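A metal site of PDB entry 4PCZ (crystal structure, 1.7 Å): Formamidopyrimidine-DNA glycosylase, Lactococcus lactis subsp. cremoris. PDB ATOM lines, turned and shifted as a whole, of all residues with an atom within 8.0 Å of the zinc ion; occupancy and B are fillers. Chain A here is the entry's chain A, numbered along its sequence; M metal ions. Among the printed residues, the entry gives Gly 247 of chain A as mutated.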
ATOM      1  N   TRP A 179       7.932 -23.649  22.029  1.00  0.00           N
ATOM      2  CA  TRP A 179       6.837 -24.321  21.334  1.00  0.00           C
ATOM      3  C   TRP A 179       7.398 -25.314  20.292  1.00  0.00           C
ATOM      4  O   TRP A 179       6.956 -26.460  20.182  1.00  0.00           O
ATOM      5  CB  TRP A 179       5.912 -23.262  20.688  1.00  0.00           C
ATOM      6  CG  TRP A 179       4.796 -23.922  19.864  1.00  0.00           C
ATOM      7  CD1 TRP A 179       3.537 -24.254  20.307  1.00  0.00           C
ATOM      8  CD2 TRP A 179       4.861 -24.307  18.489  1.00  0.00           C
ATOM      9  NE1 TRP A 179       2.824 -24.838  19.287  1.00  0.00           N
ATOM     10  CE2 TRP A 179       3.583 -24.869  18.156  1.00  0.00           C
ATOM     11  CE3 TRP A 179       5.830 -24.221  17.511  1.00  0.00           C
ATOM     12  CZ2 TRP A 179       3.291 -25.352  16.873  1.00  0.00           C
ATOM     13  CZ3 TRP A 179       5.544 -24.713  16.230  1.00  0.00           C
ATOM     14  CH2 TRP A 179       4.265 -25.271  15.919  1.00  0.00           C
ATOM     15  N   LYS A 182       8.653 -28.368  22.015  1.00  0.00           N
ATOM     16  CA  LYS A 182       7.641 -29.045  22.812  1.00  0.00           C
ATOM     17  C   LYS A 182       7.925 -29.064  24.304  1.00  0.00           C
ATOM     18  O   LYS A 182       7.750 -30.080  24.981  1.00  0.00           O
ATOM     19  CB  LYS A 182       7.421 -30.488  22.302  1.00  0.00           C
ATOM     20  CG  LYS A 182       7.260 -30.532  20.747  1.00  0.00           C
ATOM     21  CD  LYS A 182       6.153 -29.632  20.232  1.00  0.00           C
ATOM     22  CE  LYS A 182       6.371 -29.161  18.745  1.00  0.00           C
ATOM     23  NZ  LYS A 182       5.533 -27.933  18.259  1.00  0.00           N
ATOM     24  N   VAL A 237       3.302 -18.849  18.342  1.00  0.00           N
ATOM     25  CA  VAL A 237       2.690 -18.632  19.649  1.00  0.00           C
ATOM     26  C   VAL A 237       2.779 -17.201  20.166  1.00  0.00           C
ATOM     27  O   VAL A 237       1.849 -16.737  20.811  1.00  0.00           O
ATOM     28  CB  VAL A 237       3.270 -19.588  20.738  1.00  0.00           C
ATOM     29  CG1 VAL A 237       2.830 -21.015  20.462  1.00  0.00           C
ATOM     30  CG2 VAL A 237       4.818 -19.522  20.810  1.00  0.00           C
ATOM     31  N   LYS A 244      -5.623 -20.658  17.519  1.00  0.00           N
ATOM     32  CA  LYS A 244      -5.487 -22.121  17.640  1.00  0.00           C
ATOM     33  C   LYS A 244      -4.065 -22.525  17.288  1.00  0.00           C
ATOM     34  O   LYS A 244      -3.487 -22.014  16.342  1.00  0.00           O
ATOM     35  CB  LYS A 244      -6.456 -22.866  16.738  1.00  0.00           C
ATOM     36  CG  LYS A 244      -7.915 -22.559  17.017  1.00  0.00           C
ATOM     37  CD  LYS A 244      -8.323 -22.599  18.506  1.00  0.00           C
ATOM     38  CE  LYS A 244      -9.866 -22.319  18.600  1.00  0.00           C
ATOM     39  NZ  LYS A 244     -10.533 -22.358  19.962  1.00  0.00           N
ATOM     40  N   CYS A 245      -3.488 -23.413  18.086  1.00  0.00           N
ATOM     41  CA  CYS A 245      -2.158 -23.972  17.817  1.00  0.00           C
ATOM     42  C   CYS A 245      -2.118 -24.609  16.410  1.00  0.00           C
ATOM     43  O   CYS A 245      -3.040 -25.352  16.048  1.00  0.00           O
ATOM     44  CB  CYS A 245      -1.819 -25.047  18.860  1.00  0.00           C
ATOM     45  SG  CYS A 245      -0.232 -25.933  18.522  1.00  0.00           S
ATOM     46  N   SER A 246      -1.090 -24.332  15.614  1.00  0.00           N
ATOM     47  CA  SER A 246      -1.066 -24.947  14.258  1.00  0.00           C
ATOM     48  C   SER A 246      -0.773 -26.436  14.325  1.00  0.00           C
ATOM     49  O   SER A 246      -0.963 -27.161  13.366  1.00  0.00           O
ATOM     50  CB  SER A 246      -0.034 -24.284  13.369  1.00  0.00           C
ATOM     51  OG  SER A 246       1.264 -24.549  13.884  1.00  0.00           O
ATOM     52  N   GLY A 247      -0.266 -26.889  15.454  1.00  0.00           N
ATOM     53  CA  GLY A 247       0.080 -28.296  15.587  1.00  0.00           C
ATOM     54  C   GLY A 247      -1.050 -29.167  16.065  1.00  0.00           C
ATOM     55  O   GLY A 247      -1.156 -30.324  15.652  1.00  0.00           O
ATOM     56  N   CYS A 248      -1.910 -28.644  16.925  1.00  0.00           N
ATOM     57  CA  CYS A 248      -2.945 -29.519  17.510  1.00  0.00           C
ATOM     58  C   CYS A 248      -4.335 -28.915  17.626  1.00  0.00           C
ATOM     59  O   CYS A 248      -5.250 -29.624  18.010  1.00  0.00           O
ATOM     60  CB  CYS A 248      -2.519 -29.954  18.915  1.00  0.00           C
ATOM     61  SG  CYS A 248      -2.583 -28.620  20.100  1.00  0.00           S
ATOM     62  N   GLY A 249      -4.468 -27.614  17.398  1.00  0.00           N
ATOM     63  CA  GLY A 249      -5.742 -26.930  17.542  1.00  0.00           C
ATOM     64  C   GLY A 249      -6.197 -26.463  18.918  1.00  0.00           C
ATOM     65  O   GLY A 249      -7.271 -25.868  19.042  1.00  0.00           O
ATOM     66  N   ALA A 250      -5.428 -26.720  19.969  1.00  0.00           N
ATOM     67  CA  ALA A 250      -5.726 -26.171  21.294  1.00  0.00           C
ATOM     68  C   ALA A 250      -5.566 -24.669  21.178  1.00  0.00           C
ATOM     69  O   ALA A 250      -4.686 -24.228  20.425  1.00  0.00           O
ATOM     70  CB  ALA A 250      -4.746 -26.735  22.356  1.00  0.00           C
ATOM     71  N   GLU A 251      -6.306 -23.887  21.959  1.00  0.00           N
ATOM     72  CA  GLU A 251      -5.964 -22.448  22.049  1.00  0.00           C
ATOM     73  C   GLU A 251      -4.646 -22.161  22.741  1.00  0.00           C
ATOM     74  O   GLU A 251      -4.337 -22.664  23.853  1.00  0.00           O
ATOM     75  CB  GLU A 251      -7.031 -21.634  22.788  1.00  0.00           C
ATOM     76  CG  GLU A 251      -8.318 -21.710  22.147  1.00  0.00           C
ATOM     77  CD  GLU A 251      -9.261 -20.585  22.528  1.00  0.00           C
ATOM     78  OE1 GLU A 251      -9.013 -19.784  23.499  1.00  0.00           O
ATOM     79  OE2 GLU A 251     -10.240 -20.487  21.782  1.00  0.00           O
ATOM     80  N   ILE A 252      -3.874 -21.286  22.115  1.00  0.00           N
ATOM     81  CA  ILE A 252      -2.675 -20.745  22.774  1.00  0.00           C
ATOM     82  C   ILE A 252      -3.060 -19.962  24.034  1.00  0.00           C
ATOM     83  O   ILE A 252      -3.982 -19.141  24.044  1.00  0.00           O
ATOM     84  CB  ILE A 252      -1.887 -19.839  21.773  1.00  0.00           C
ATOM     85  CG1 ILE A 252      -1.453 -20.671  20.540  1.00  0.00           C
ATOM     86  CG2 ILE A 252      -0.713 -19.097  22.502  1.00  0.00           C
ATOM     87  CD1 ILE A 252      -0.679 -22.054  20.857  1.00  0.00           C
ATOM     88  N   PHE A 264       2.060 -20.137  25.122  1.00  0.00           N
ATOM     89  CA  PHE A 264       2.414 -21.544  24.862  1.00  0.00           C
ATOM     90  C   PHE A 264       1.187 -22.345  24.489  1.00  0.00           C
ATOM     91  O   PHE A 264       0.043 -21.935  24.723  1.00  0.00           O
ATOM     92  CB  PHE A 264       3.077 -22.152  26.119  1.00  0.00           C
ATOM     93  CG  PHE A 264       2.108 -22.355  27.259  1.00  0.00           C
ATOM     94  CD1 PHE A 264       1.647 -21.265  27.983  1.00  0.00           C
ATOM     95  CD2 PHE A 264       1.646 -23.635  27.576  1.00  0.00           C
ATOM     96  CE1 PHE A 264       0.727 -21.432  29.006  1.00  0.00           C
ATOM     97  CE2 PHE A 264       0.711 -23.813  28.592  1.00  0.00           C
ATOM     98  CZ  PHE A 264       0.272 -22.707  29.327  1.00  0.00           C
ATOM     99  N   CYS A 265       1.415 -23.507  23.895  1.00  0.00           N
ATOM    100  CA  CYS A 265       0.323 -24.467  23.694  1.00  0.00           C
ATOM    101  C   CYS A 265       0.305 -25.483  24.838  1.00  0.00           C
ATOM    102  O   CYS A 265       1.273 -26.189  25.039  1.00  0.00           O
ATOM    103  CB  CYS A 265       0.523 -25.224  22.388  1.00  0.00           C
ATOM    104  SG  CYS A 265      -0.784 -26.516  22.215  1.00  0.00           S
ATOM    105  N   PRO A 266      -0.800 -25.585  25.610  1.00  0.00           N
ATOM    106  CA  PRO A 266      -0.821 -26.532  26.739  1.00  0.00           C
ATOM    107  C   PRO A 266      -0.809 -27.987  26.320  1.00  0.00           C
ATOM    108  O   PRO A 266      -0.544 -28.815  27.184  1.00  0.00           O
ATOM    109  CB  PRO A 266      -2.173 -26.252  27.437  1.00  0.00           C
ATOM    110  CG  PRO A 266      -2.663 -25.021  26.832  1.00  0.00           C
ATOM    111  CD  PRO A 266      -2.026 -24.776  25.516  1.00  0.00           C
ATOM    112  N   VAL A 267      -1.134 -28.292  25.078  1.00  0.00           N
ATOM    113  CA  VAL A 267      -1.081 -29.686  24.575  1.00  0.00           C
ATOM    114  C   VAL A 267       0.321 -30.061  24.119  1.00  0.00           C
ATOM    115  O   VAL A 267       0.937 -31.085  24.531  1.00  0.00           O
ATOM    116  CB  VAL A 267      -2.072 -29.892  23.444  1.00  0.00           C
ATOM    117  CG1 VAL A 267      -1.878 -31.252  22.810  1.00  0.00           C
ATOM    118  CG2 VAL A 267      -3.503 -29.888  24.040  1.00  0.00           C
ATOM    119  N   CYS A 268       0.883 -29.231  23.261  1.00  0.00           N
ATOM    120  CA  CYS A 268       2.183 -29.508  22.706  1.00  0.00           C
ATOM    121  C   CYS A 268       3.352 -29.283  23.686  1.00  0.00           C
ATOM    122  O   CYS A 268       4.413 -29.844  23.462  1.00  0.00           O
ATOM    123  CB  CYS A 268       2.409 -28.666  21.445  1.00  0.00           C
ATOM    124  SG  CYS A 268       1.215 -29.066  20.101  1.00  0.00           S
ATOM    125  N   GLN A 269       3.121 -28.492  24.751  1.00  0.00           N
ATOM    126  CA  GLN A 269       4.166 -28.146  25.714  1.00  0.00           C
ATOM    127  C   GLN A 269       3.629 -28.582  27.085  1.00  0.00           C
ATOM    128  O   GLN A 269       3.083 -27.762  27.836  1.00  0.00           O
ATOM    129  CB  GLN A 269       4.488 -26.655  25.692  1.00  0.00           C
ATOM    130  CG  GLN A 269       5.000 -26.223  24.321  1.00  0.00           C
ATOM    131  CD  GLN A 269       5.008 -24.674  24.220  1.00  0.00           C
ATOM    132  OE1 GLN A 269       4.123 -24.095  23.588  1.00  0.00           O
ATOM    133  NE2 GLN A 269       6.008 -24.024  24.870  1.00  0.00           N
HETATM  134 ZN    ZN M   1      -0.522 -27.586  20.170  1.00  0.00          ZN
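The side-chain sulfur of Cys 248 lies close to the backbone NH of Ala 250 (3.4 Å). The side-chain sulfur (SG) of Cys 265 lies close to the backbone NH (N) of Val 267 (3.4 Å). The backbone NH of Cys 265 lies within hydrogen-bond range of the side-chain amide oxygen of Gln 269. NE1 of Trp 179 lies close to SG of Cys 245, 3.3 Å away. The side-chain sulfur (SG) of Cys 245 sits close to the backbone NH (N) of Gly 247 (3.2 Å). N of Cys 245 sits at hydrogen-bond distance from O of Ala 250.
The nearest printed residue that does not touch the zinc ion is Val 267 (4.3 Å).
The zinc ion is bound by SG of Cys 268 (2.3 Å), SG of Cys 248 (2.3 Å), SG of Cys 265 (2.3 Å) and SG of Cys 245 (2.4 Å).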
